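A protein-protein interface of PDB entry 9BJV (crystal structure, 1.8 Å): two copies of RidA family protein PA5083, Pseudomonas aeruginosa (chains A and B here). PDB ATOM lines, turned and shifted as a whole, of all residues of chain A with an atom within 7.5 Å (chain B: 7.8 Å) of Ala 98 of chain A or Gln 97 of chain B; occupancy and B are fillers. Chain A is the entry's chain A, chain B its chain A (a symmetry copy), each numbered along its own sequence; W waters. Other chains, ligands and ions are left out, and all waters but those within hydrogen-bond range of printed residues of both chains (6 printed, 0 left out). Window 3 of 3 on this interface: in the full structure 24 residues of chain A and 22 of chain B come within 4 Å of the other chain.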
ATOM      1  N   ILE A  65       2.318  15.507   6.521  1.00  0.00           N
ATOM      2  CA  ILE A  65       1.831  16.432   7.542  1.00  0.00           C
ATOM      3  C   ILE A  65       0.462  16.927   7.099  1.00  0.00           C
ATOM      4  O   ILE A  65       0.342  17.582   6.059  1.00  0.00           O
ATOM      5  CB  ILE A  65       2.813  17.602   7.742  1.00  0.00           C
ATOM      6  CG1 ILE A  65       4.176  17.069   8.195  1.00  0.00           C
ATOM      7  CG2 ILE A  65       2.263  18.613   8.750  1.00  0.00           C
ATOM      8  CD1 ILE A  65       5.236  18.168   8.459  1.00  0.00           C
ATOM      9  N   TYR A  66      -0.569  16.605   7.872  1.00  0.00           N
ATOM     10  CA  TYR A  66      -1.927  17.066   7.591  1.00  0.00           C
ATOM     11  C   TYR A  66      -2.230  18.252   8.494  1.00  0.00           C
ATOM     12  O   TYR A  66      -2.072  18.153   9.716  1.00  0.00           O
ATOM     13  CB  TYR A  66      -2.956  15.963   7.844  1.00  0.00           C
ATOM     14  CG  TYR A  66      -2.742  14.703   7.024  1.00  0.00           C
ATOM     15  CD1 TYR A  66      -3.231  14.613   5.721  1.00  0.00           C
ATOM     16  CD2 TYR A  66      -2.071  13.603   7.557  1.00  0.00           C
ATOM     17  CE1 TYR A  66      -3.050  13.454   4.957  1.00  0.00           C
ATOM     18  CE2 TYR A  66      -1.880  12.436   6.801  1.00  0.00           C
ATOM     19  CZ  TYR A  66      -2.377  12.378   5.504  1.00  0.00           C
ATOM     20  OH  TYR A  66      -2.198  11.235   4.756  1.00  0.00           O
ATOM     21  N   LEU A  67      -2.654  19.367   7.894  1.00  0.00           N
ATOM     22  CA  LEU A  67      -3.073  20.547   8.644  1.00  0.00           C
ATOM     23  C   LEU A  67      -4.547  20.818   8.388  1.00  0.00           C
ATOM     24  O   LEU A  67      -5.003  20.780   7.240  1.00  0.00           O
ATOM     25  CB  LEU A  67      -2.247  21.780   8.261  1.00  0.00           C
ATOM     26  CG  LEU A  67      -0.782  21.682   8.686  1.00  0.00           C
ATOM     27  CD1 LEU A  67       0.068  22.754   8.030  1.00  0.00           C
ATOM     28  CD2 LEU A  67      -0.706  21.774  10.200  1.00  0.00           C
ATOM     29  N   LYS A  68      -5.292  21.110   9.455  1.00  0.00           N
ATOM     30  CA  LYS A  68      -6.703  21.440   9.270  1.00  0.00           C
ATOM     31  C   LYS A  68      -6.865  22.732   8.478  1.00  0.00           C
ATOM     32  O   LYS A  68      -7.761  22.840   7.634  1.00  0.00           O
ATOM     33  CB  LYS A  68      -7.413  21.539  10.621  1.00  0.00           C
ATOM     34  CG  LYS A  68      -8.936  21.704  10.523  1.00  0.00           C
ATOM     35  CD  LYS A  68      -9.523  22.047  11.880  1.00  0.00           C
ATOM     36  CE  LYS A  68     -11.046  21.875  11.907  1.00  0.00           C
ATOM     37  NZ  LYS A  68     -11.733  22.850  11.025  1.00  0.00           N
ATOM     38  N   ASP A  69      -5.993  23.712   8.716  1.00  0.00           N
ATOM     39  CA  ASP A  69      -6.013  24.989   7.998  1.00  0.00           C
ATOM     40  C   ASP A  69      -4.586  25.291   7.564  1.00  0.00           C
ATOM     41  O   ASP A  69      -3.810  25.913   8.298  1.00  0.00           O
ATOM     42  CB  ASP A  69      -6.582  26.111   8.856  1.00  0.00           C
ATOM     43  CG  ASP A  69      -6.861  27.371   8.051  1.00  0.00           C
ATOM     44  OD1 ASP A  69      -6.111  27.670   7.097  1.00  0.00           O
ATOM     45  OD2 ASP A  69      -7.838  28.071   8.369  1.00  0.00           O
ATOM     46  N   ILE A  70      -4.245  24.874   6.348  1.00  0.00           N
ATOM     47  CA  ILE A  70      -2.862  24.987   5.919  1.00  0.00           C
ATOM     48  C   ILE A  70      -2.464  26.453   5.757  1.00  0.00           C
ATOM     49  O   ILE A  70      -1.340  26.840   6.092  1.00  0.00           O
ATOM     50  CB  ILE A  70      -2.629  24.147   4.645  1.00  0.00           C
ATOM     51  CG1 ILE A  70      -1.133  23.995   4.373  1.00  0.00           C
ATOM     52  CG2 ILE A  70      -3.370  24.724   3.420  1.00  0.00           C
ATOM     53  CD1 ILE A  70      -0.817  22.817   3.459  1.00  0.00           C
ATOM     54  N   VAL A  96      -0.251  18.830   3.429  1.00  0.00           N
ATOM     55  CA  VAL A  96      -1.523  19.073   2.757  1.00  0.00           C
ATOM     56  C   VAL A  96      -2.584  19.410   3.789  1.00  0.00           C
ATOM     57  O   VAL A  96      -2.439  19.144   4.986  1.00  0.00           O
ATOM     58  CB  VAL A  96      -1.998  17.870   1.914  1.00  0.00           C
ATOM     59  CG1 VAL A  96      -0.935  17.458   0.931  1.00  0.00           C
ATOM     60  CG2 VAL A  96      -2.403  16.711   2.824  1.00  0.00           C
ATOM     61  N   GLN A  97      -3.681  19.975   3.300  1.00  0.00           N
ATOM     62  CA  GLN A  97      -4.803  20.300   4.165  1.00  0.00           C
ATOM     63  C   GLN A  97      -5.786  19.137   4.210  1.00  0.00           C
ATOM     64  O   GLN A  97      -6.157  18.582   3.168  1.00  0.00           O
ATOM     65  CB  GLN A  97      -5.514  21.564   3.692  1.00  0.00           C
ATOM     66  CG  GLN A  97      -6.669  21.985   4.599  1.00  0.00           C
ATOM     67  CD  GLN A  97      -7.171  23.368   4.265  1.00  0.00           C
ATOM     68  OE1 GLN A  97      -6.538  24.368   4.609  1.00  0.00           O
ATOM     69  NE2 GLN A  97      -8.299  23.437   3.559  1.00  0.00           N
ATOM     70  N   ALA A  98      -6.207  18.771   5.420  1.00  0.00           N
ATOM     71  CA  ALA A  98      -7.246  17.765   5.576  1.00  0.00           C
ATOM     72  C   ALA A  98      -7.854  17.928   6.956  1.00  0.00           C
ATOM     73  O   ALA A  98      -7.152  18.259   7.914  1.00  0.00           O
ATOM     74  CB  ALA A  98      -6.701  16.339   5.410  1.00  0.00           C
ATOM     75  N   GLU A  99      -9.157  17.709   7.046  1.00  0.00           N
ATOM     76  CA  GLU A  99      -9.795  17.642   8.348  1.00  0.00           C
ATOM     77  C   GLU A  99      -9.430  16.324   9.024  1.00  0.00           C
ATOM     78  O   GLU A  99      -9.375  15.272   8.380  1.00  0.00           O
ATOM     79  CB  GLU A  99     -11.306  17.767   8.190  1.00  0.00           C
ATOM     80  CG  GLU A  99     -12.043  17.770   9.496  1.00  0.00           C
ATOM     81  CD  GLU A  99     -12.517  19.148   9.869  1.00  0.00           C
ATOM     82  OE1 GLU A  99     -12.085  20.129   9.207  1.00  0.00           O
ATOM     83  OE2 GLU A  99     -13.322  19.240  10.823  1.00  0.00           O
ATOM     84  N   LEU A 100      -9.156  16.379  10.326  1.00  0.00           N
ATOM     85  CA  LEU A 100      -8.805  15.185  11.075  1.00  0.00           C
ATOM     86  C   LEU A 100     -10.037  14.681  11.825  1.00  0.00           C
ATOM     87  O   LEU A 100     -11.130  15.238  11.712  1.00  0.00           O
ATOM     88  CB  LEU A 100      -7.619  15.459  12.006  1.00  0.00           C
ATOM     89  CG  LEU A 100      -6.275  15.763  11.307  1.00  0.00           C
ATOM     90  CD1 LEU A 100      -6.096  14.953  10.001  1.00  0.00           C
ATOM     91  CD2 LEU A 100      -6.039  17.265  11.052  1.00  0.00           C
ATOM     92  N   ALA A 101      -9.863  13.606  12.601  1.00  0.00           N
ATOM     93  CA  ALA A 101     -11.037  12.916  13.148  1.00  0.00           C
ATOM     94  C   ALA A 101     -11.816  13.777  14.141  1.00  0.00           C
ATOM     95  O   ALA A 101     -13.025  13.577  14.316  1.00  0.00           O
ATOM     96  CB  ALA A 101     -10.624  11.598  13.806  1.00  0.00           C
ATOM     97  N   VAL A 105      -8.516  19.016  16.368  1.00  0.00           N
ATOM     98  CA  VAL A 105      -7.174  18.603  15.965  1.00  0.00           C
ATOM     99  C   VAL A 105      -6.740  19.445  14.770  1.00  0.00           C
ATOM    100  O   VAL A 105      -7.403  19.451  13.727  1.00  0.00           O
ATOM    101  CB  VAL A 105      -7.127  17.105  15.636  1.00  0.00           C
ATOM    102  CG1 VAL A 105      -5.746  16.733  15.090  1.00  0.00           C
ATOM    103  CG2 VAL A 105      -7.446  16.287  16.886  1.00  0.00           C
ATOM    104  N   LEU A 106      -5.623  20.152  14.918  1.00  0.00           N
ATOM    105  CA  LEU A 106      -5.142  21.049  13.876  1.00  0.00           C
ATOM    106  C   LEU A 106      -4.053  20.433  13.020  1.00  0.00           C
ATOM    107  O   LEU A 106      -3.758  20.966  11.945  1.00  0.00           O
ATOM    108  CB  LEU A 106      -4.592  22.341  14.487  1.00  0.00           C
ATOM    109  CG  LEU A 106      -5.568  23.133  15.366  1.00  0.00           C
ATOM    110  CD1 LEU A 106      -4.875  24.359  15.937  1.00  0.00           C
ATOM    111  CD2 LEU A 106      -6.807  23.536  14.567  1.00  0.00           C
ATOM    112  N   VAL A 107      -3.428  19.362  13.494  1.00  0.00           N
ATOM    113  CA  VAL A 107      -2.239  18.806  12.861  1.00  0.00           C
ATOM    114  C   VAL A 107      -2.180  17.318  13.187  1.00  0.00           C
ATOM    115  O   VAL A 107      -2.481  16.903  14.311  1.00  0.00           O
ATOM    116  CB  VAL A 107      -0.971  19.558  13.325  1.00  0.00           C
ATOM    117  CG1 VAL A 107      -0.871  19.593  14.876  1.00  0.00           C
ATOM    118  CG2 VAL A 107       0.289  18.965  12.693  1.00  0.00           C
ATOM    119  N   GLU A 108      -1.826  16.512  12.181  1.00  0.00           N
ATOM    120  CA  GLU A 108      -1.583  15.084  12.338  1.00  0.00           C
ATOM    121  C   GLU A 108      -0.444  14.709  11.404  1.00  0.00           C
ATOM    122  O   GLU A 108      -0.386  15.206  10.277  1.00  0.00           O
ATOM    123  CB  GLU A 108      -2.835  14.235  12.021  1.00  0.00           C
ATOM    124  CG  GLU A 108      -2.564  12.698  12.095  1.00  0.00           C
ATOM    125  CD  GLU A 108      -3.826  11.841  12.128  1.00  0.00           C
ATOM    126  OE1 GLU A 108      -4.927  12.411  12.302  1.00  0.00           O
ATOM    127  OE2 GLU A 108      -3.721  10.586  11.983  1.00  0.00           O
ATOM    128  N   ILE B  65      -6.815   5.853   5.405  1.00  0.00           N
ATOM    129  CA  ILE B  65      -8.259   5.779   5.200  1.00  0.00           C
ATOM    130  C   ILE B  65      -8.760   7.192   4.934  1.00  0.00           C
ATOM    131  O   ILE B  65      -8.653   8.064   5.801  1.00  0.00           O
ATOM    132  CB  ILE B  65      -8.961   5.156   6.421  1.00  0.00           C
ATOM    133  CG1 ILE B  65      -8.441   3.733   6.654  1.00  0.00           C
ATOM    134  CG2 ILE B  65     -10.480   5.155   6.239  1.00  0.00           C
ATOM    135  CD1 ILE B  65      -9.105   2.996   7.844  1.00  0.00           C
ATOM    136  N   TYR B  66      -9.289   7.424   3.738  1.00  0.00           N
ATOM    137  CA  TYR B  66      -9.859   8.720   3.376  1.00  0.00           C
ATOM    138  C   TYR B  66     -11.372   8.634   3.504  1.00  0.00           C
ATOM    139  O   TYR B  66     -11.990   7.735   2.922  1.00  0.00           O
ATOM    140  CB  TYR B  66      -9.494   9.112   1.944  1.00  0.00           C
ATOM    141  CG  TYR B  66      -8.002   9.198   1.675  1.00  0.00           C
ATOM    142  CD1 TYR B  66      -7.292  10.358   1.983  1.00  0.00           C
ATOM    143  CD2 TYR B  66      -7.312   8.131   1.101  1.00  0.00           C
ATOM    144  CE1 TYR B  66      -5.919  10.456   1.731  1.00  0.00           C
ATOM    145  CE2 TYR B  66      -5.934   8.215   0.846  1.00  0.00           C
ATOM    146  CZ  TYR B  66      -5.254   9.384   1.167  1.00  0.00           C
ATOM    147  OH  TYR B  66      -3.901   9.477   0.916  1.00  0.00           O
ATOM    148  N   LEU B  67     -11.961   9.558   4.267  1.00  0.00           N
ATOM    149  CA  LEU B  67     -13.411   9.654   4.398  1.00  0.00           C
ATOM    150  C   LEU B  67     -13.889  10.983   3.835  1.00  0.00           C
ATOM    151  O   LEU B  67     -13.301  12.032   4.118  1.00  0.00           O
ATOM    152  CB  LEU B  67     -13.854   9.523   5.860  1.00  0.00           C
ATOM    153  CG  LEU B  67     -13.609   8.132   6.444  1.00  0.00           C
ATOM    154  CD1 LEU B  67     -13.760   8.120   7.954  1.00  0.00           C
ATOM    155  CD2 LEU B  67     -14.569   7.153   5.790  1.00  0.00           C
ATOM    156  N   LYS B  68     -14.967  10.944   3.051  1.00  0.00           N
ATOM    157  CA  LYS B  68     -15.513  12.193   2.528  1.00  0.00           C
ATOM    158  C   LYS B  68     -16.041  13.076   3.652  1.00  0.00           C
ATOM    159  O   LYS B  68     -15.874  14.299   3.618  1.00  0.00           O
ATOM    160  CB  LYS B  68     -16.609  11.911   1.499  1.00  0.00           C
ATOM    161  CG  LYS B  68     -17.119  13.156   0.761  1.00  0.00           C
ATOM    162  CD  LYS B  68     -18.364  12.829  -0.043  1.00  0.00           C
ATOM    163  CE  LYS B  68     -18.698  13.927  -1.058  1.00  0.00           C
ATOM    164  NZ  LYS B  68     -19.090  15.196  -0.399  1.00  0.00           N
ATOM    165  N   ASP B  69     -16.657  12.473   4.669  1.00  0.00           N
ATOM    166  CA  ASP B  69     -17.177  13.198   5.831  1.00  0.00           C
ATOM    167  C   ASP B  69     -16.722  12.452   7.077  1.00  0.00           C
ATOM    168  O   ASP B  69     -17.399  11.539   7.561  1.00  0.00           O
ATOM    169  CB  ASP B  69     -18.693  13.328   5.784  1.00  0.00           C
ATOM    170  CG  ASP B  69     -19.224  14.301   6.827  1.00  0.00           C
ATOM    171  OD1 ASP B  69     -18.651  14.388   7.933  1.00  0.00           O
ATOM    172  OD2 ASP B  69     -20.221  14.985   6.542  1.00  0.00           O
ATOM    173  N   ILE B  70     -15.579  12.863   7.619  1.00  0.00           N
ATOM    174  CA  ILE B  70     -15.000  12.108   8.715  1.00  0.00           C
ATOM    175  C   ILE B  70     -15.873  12.212   9.965  1.00  0.00           C
ATOM    176  O   ILE B  70     -16.033  11.235  10.703  1.00  0.00           O
ATOM    177  CB  ILE B  70     -13.540  12.549   8.953  1.00  0.00           C
ATOM    178  CG1 ILE B  70     -12.825  11.557   9.870  1.00  0.00           C
ATOM    179  CG2 ILE B  70     -13.445  13.991   9.500  1.00  0.00           C
ATOM    180  CD1 ILE B  70     -11.307  11.642   9.760  1.00  0.00           C
ATOM    181  N   ALA B  71     -16.488  13.374  10.211  1.00  0.00           N
ATOM    182  CA  ALA B  71     -17.329  13.490  11.401  1.00  0.00           C
ATOM    183  C   ALA B  71     -18.517  12.538  11.327  1.00  0.00           C
ATOM    184  O   ALA B  71     -18.883  11.900  12.322  1.00  0.00           O
ATOM    185  CB  ALA B  71     -17.807  14.937  11.575  1.00  0.00           C
ATOM    186  N   ARG B  72     -19.111  12.408  10.145  1.00  0.00           N
ATOM    187  CA  ARG B  72     -20.339  11.645  10.003  1.00  0.00           C
ATOM    188  C   ARG B  72     -20.084  10.144   9.970  1.00  0.00           C
ATOM    189  O   ARG B  72     -20.888   9.364  10.495  1.00  0.00           O
ATOM    190  CB  ARG B  72     -21.039  12.081   8.723  1.00  0.00           C
ATOM    191  CG  ARG B  72     -22.374  11.447   8.457  1.00  0.00           C
ATOM    192  CD  ARG B  72     -22.921  12.134   7.248  1.00  0.00           C
ATOM    193  NE  ARG B  72     -24.305  11.802   6.947  1.00  0.00           N
ATOM    194  CZ  ARG B  72     -25.025  12.482   6.072  1.00  0.00           C
ATOM    195  NH1 ARG B  72     -24.526  13.539   5.448  1.00  0.00           N
ATOM    196  NH2 ARG B  72     -26.270  12.091   5.812  1.00  0.00           N
ATOM    197  N   ASP B  73     -18.983   9.725   9.345  1.00  0.00           N
ATOM    198  CA  ASP B  73     -18.790   8.333   8.952  1.00  0.00           C
ATOM    199  C   ASP B  73     -17.679   7.617   9.713  1.00  0.00           C
ATOM    200  O   ASP B  73     -17.500   6.409   9.523  1.00  0.00           O
ATOM    201  CB  ASP B  73     -18.520   8.259   7.442  1.00  0.00           C
ATOM    202  CG  ASP B  73     -19.756   8.564   6.627  1.00  0.00           C
ATOM    203  OD1 ASP B  73     -20.864   8.362   7.162  1.00  0.00           O
ATOM    204  OD2 ASP B  73     -19.632   8.995   5.458  1.00  0.00           O
ATOM    205  N   THR B  94      -3.861   5.773   9.354  1.00  0.00           N
ATOM    206  CA  THR B  94      -4.106   7.209   9.385  1.00  0.00           C
ATOM    207  C   THR B  94      -5.461   7.448   8.738  1.00  0.00           C
ATOM    208  O   THR B  94      -5.694   6.961   7.632  1.00  0.00           O
ATOM    209  CB  THR B  94      -3.015   7.979   8.625  1.00  0.00           C
ATOM    210  OG1 THR B  94      -1.740   7.736   9.224  1.00  0.00           O
ATOM    211  CG2 THR B  94      -3.298   9.471   8.627  1.00  0.00           C
ATOM    212  N   THR B  95      -6.351   8.182   9.416  1.00  0.00           N
ATOM    213  CA  THR B  95      -7.703   8.440   8.925  1.00  0.00           C
ATOM    214  C   THR B  95      -7.889   9.944   8.783  1.00  0.00           C
ATOM    215  O   THR B  95      -7.772  10.680   9.767  1.00  0.00           O
ATOM    216  CB  THR B  95      -8.765   7.868   9.875  1.00  0.00           C
ATOM    217  OG1 THR B  95      -8.440   6.514  10.199  1.00  0.00           O
ATOM    218  CG2 THR B  95     -10.139   7.891   9.211  1.00  0.00           C
ATOM    219  N   VAL B  96      -8.166  10.405   7.565  1.00  0.00           N
ATOM    220  CA  VAL B  96      -8.313  11.834   7.310  1.00  0.00           C
ATOM    221  C   VAL B  96      -9.495  12.065   6.387  1.00  0.00           C
ATOM    222  O   VAL B  96      -9.978  11.156   5.704  1.00  0.00           O
ATOM    223  CB  VAL B  96      -7.051  12.468   6.685  1.00  0.00           C
ATOM    224  CG1 VAL B  96      -5.840  12.190   7.537  1.00  0.00           C
ATOM    225  CG2 VAL B  96      -6.858  11.968   5.255  1.00  0.00           C
ATOM    226  N   GLN B  97      -9.940  13.315   6.349  1.00  0.00           N
ATOM    227  CA  GLN B  97     -11.032  13.692   5.466  1.00  0.00           C
ATOM    228  C   GLN B  97     -10.484  14.166   4.126  1.00  0.00           C
ATOM    229  O   GLN B  97      -9.551  14.979   4.075  1.00  0.00           O
ATOM    230  CB  GLN B  97     -11.891  14.786   6.092  1.00  0.00           C
ATOM    231  CG  GLN B  97     -13.090  15.182   5.231  1.00  0.00           C
ATOM    232  CD  GLN B  97     -14.061  16.056   5.985  1.00  0.00           C
ATOM    233  OE1 GLN B  97     -14.825  15.571   6.821  1.00  0.00           O
ATOM    234  NE2 GLN B  97     -14.015  17.361   5.721  1.00  0.00           N
ATOM    235  N   ALA B  98     -11.065  13.656   3.041  1.00  0.00           N
ATOM    236  CA  ALA B  98     -10.717  14.136   1.713  1.00  0.00           C
ATOM    237  C   ALA B  98     -11.848  13.772   0.769  1.00  0.00           C
ATOM    238  O   ALA B  98     -12.467  12.715   0.914  1.00  0.00           O
ATOM    239  CB  ALA B  98      -9.400  13.531   1.206  1.00  0.00           C
ATOM    240  N   GLU B  99     -12.122  14.655  -0.178  1.00  0.00           N
ATOM    241  CA  GLU B  99     -13.043  14.315  -1.245  1.00  0.00           C
ATOM    242  C   GLU B  99     -12.367  13.345  -2.210  1.00  0.00           C
ATOM    243  O   GLU B  99     -11.182  13.486  -2.527  1.00  0.00           O
ATOM    244  CB  GLU B  99     -13.483  15.580  -1.972  1.00  0.00           C
ATOM    245  CG  GLU B  99     -14.489  15.326  -3.055  1.00  0.00           C
ATOM    246  CD  GLU B  99     -15.874  15.739  -2.641  1.00  0.00           C
ATOM    247  OE1 GLU B  99     -16.078  16.027  -1.431  1.00  0.00           O
ATOM    248  OE2 GLU B  99     -16.754  15.774  -3.530  1.00  0.00           O
ATOM    249  N   LEU B 100     -13.114  12.341  -2.665  1.00  0.00           N
ATOM    250  CA  LEU B 100     -12.577  11.363  -3.596  1.00  0.00           C
ATOM    251  C   LEU B 100     -13.016  11.723  -5.014  1.00  0.00           C
ATOM    252  O   LEU B 100     -13.681  12.735  -5.243  1.00  0.00           O
ATOM    253  CB  LEU B 100     -12.996   9.945  -3.191  1.00  0.00           C
ATOM    254  CG  LEU B 100     -12.406   9.426  -1.861  1.00  0.00           C
ATOM    255  CD1 LEU B 100     -10.965   9.934  -1.619  1.00  0.00           C
ATOM    256  CD2 LEU B 100     -13.298   9.718  -0.636  1.00  0.00           C
HETATM  257  O   HOH W   1      -5.656   8.962  12.080  1.00  0.00           O
HETATM  258  O   HOH W   2      -2.167  11.048   2.128  1.00  0.00           O
HETATM  259  O   HOH W   3      -7.628  11.812  12.178  1.00  0.00           O
HETATM  260  O   HOH W   4      -8.411  16.947   2.196  1.00  0.00           O
HETATM  261  O   HOH W   5     -15.135  11.971  13.706  1.00  0.00           O
HETATM  262  O   HOH W   6     -10.591  17.936   4.426  1.00  0.00           O
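Tyr 66 of chain A touches Val 96 of chain B, but with the chains exchanged Val 96 of chain A does not touch Tyr 66 of chain B (7.3 Å). Glu 99 of chain A touches Val 96 of chain B, but with the chains exchanged Val 96 of chain A does not touch Glu 99 of chain B (10.4 Å). Glu 99 of chain A touches Gln 97 of chain B, but with the chains exchanged Gln 97 of chain A does not touch Glu 99 of chain B (7.9 Å). Leu 100 of chain A touches Val 96 of chain B, but with the chains exchanged Val 96 of chain A does not touch Leu 100 of chain B (11.8 Å). Positions printed for both chains: 65, 66, 67, 68, 69, 70, 96, 97, 98, 99 and 100. Of the 9 pairs that touch across the chains among the printed residues, none has its exchanged pair printed and touching as well.
Water W1 lies within hydrogen-bond range of OE2 of Glu 108 of chain A (2.5 Å) and N of Thr 95 of chain B (2.9 Å). Water W2 bridges OH of Tyr 66 of chain B and OH of Tyr 66 of chain A. Water W3 lies within hydrogen-bond range of O of Thr 95 of chain B, OE1 of Glu 108 of chain A and N of Ala 101 of chain A. Water W5 bridges O of Ala 101 of chain A and O of Ile 70 of chain B. Water W4 bridges O of Gln 97 of chain A and O of Gln 97 of chain B. Water W6 lies within hydrogen-bond range of the backbone NH of Glu 99 of chain A and the backbone carbonyl oxygen of Gln 97 of chain B.
The backbone NH (N) of Leu 67 of chain B is in hydrogen-bond range of the backbone carbonyl oxygen (O) of Val 96 of chain B, at 2.9 Å. O of Leu 67 of chain A lies within hydrogen-bond range of N of Ala 98 of chain A (3.0 Å). The side-chain carboxylate (OE1) of Glu 99 of chain A lies within salt-bridge range of the side-chain amino group (NZ) of Lys 68 of chain A, 3.3 Å away. The backbone NH of Ile 70 of chain B sits at hydrogen-bond distance from the side-chain amide oxygen of Gln 97 of chain B, at 2.9 Å. N of Ile 65 of chain B lies within hydrogen-bond range of O of Thr 94 of chain B (2.7 Å). N of Tyr 66 of chain A sits at hydrogen-bond distance from O of Glu 108 of chain A (2.8 Å).
CE2 of Tyr 66 of chain A touches CG2 of Thr 94 of chain B, at 3.8 Å. Val 96 of chain B touches Tyr 66 of chain A (CG1 to CD1, 3.997 Å). Gln 97 of chain B touches Ala 98 of chain A (O to CB, 3.4 Å). CA of Val 96 of chain B touches O of Glu 99 of chain A (3.8 Å). Leu 100 of chain A touches Ile 70 of chain B (O to CG2, 3.4 Å). Leu 100 of chain A touches Val 96 of chain B (CD1 to CG1, 3.7 Å). CD1 of Ile 70 of chain B touches CA of Ala 101 of chain A, 3.6 Å away. CG2 of Thr 94 of chain B touches OE2 of Glu 108 of chain A, at 3.6 Å.
Of the 16 printed residues of chain B, 4 touch a printed residue of chain A. Printed residues of chain B that touch a printed residue of chain A: Ile 70, Thr 94, Val 96 and Gln 97. Printed residues of chain A that touch a printed residue of chain B: Tyr 66, Ala 98, Glu 99, Leu 100, Ala 101 and Glu 108. Hydrophobic or aromatic side chains of chain A that line the printed part of chain B: Tyr 66, Ala 98 and Leu 100.
The backbone carbonyl oxygen of Glu 99 of chain A lies within hydrogen-bond range of the backbone NH of Gln 97 of chain B, at 2.9 Å.
Of chain A, only Ala 98 (3.4 Å) and Glu 99 (2.9 Å) come within 4 Å of Gln 97 of chain B. Printed residues of chain B within 4 Å of Ala 101 of chain A: Ile 70. Printed residues of chain B within 4 Å of Glu 99 of chain A: Val 96 and Gln 97. Lys 68 of chain B touches none of the printed residues of chain A. The nearest residue of chain A that does not touch Gln 97 of chain B is Gln 97 of chain A (5.0 Å).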
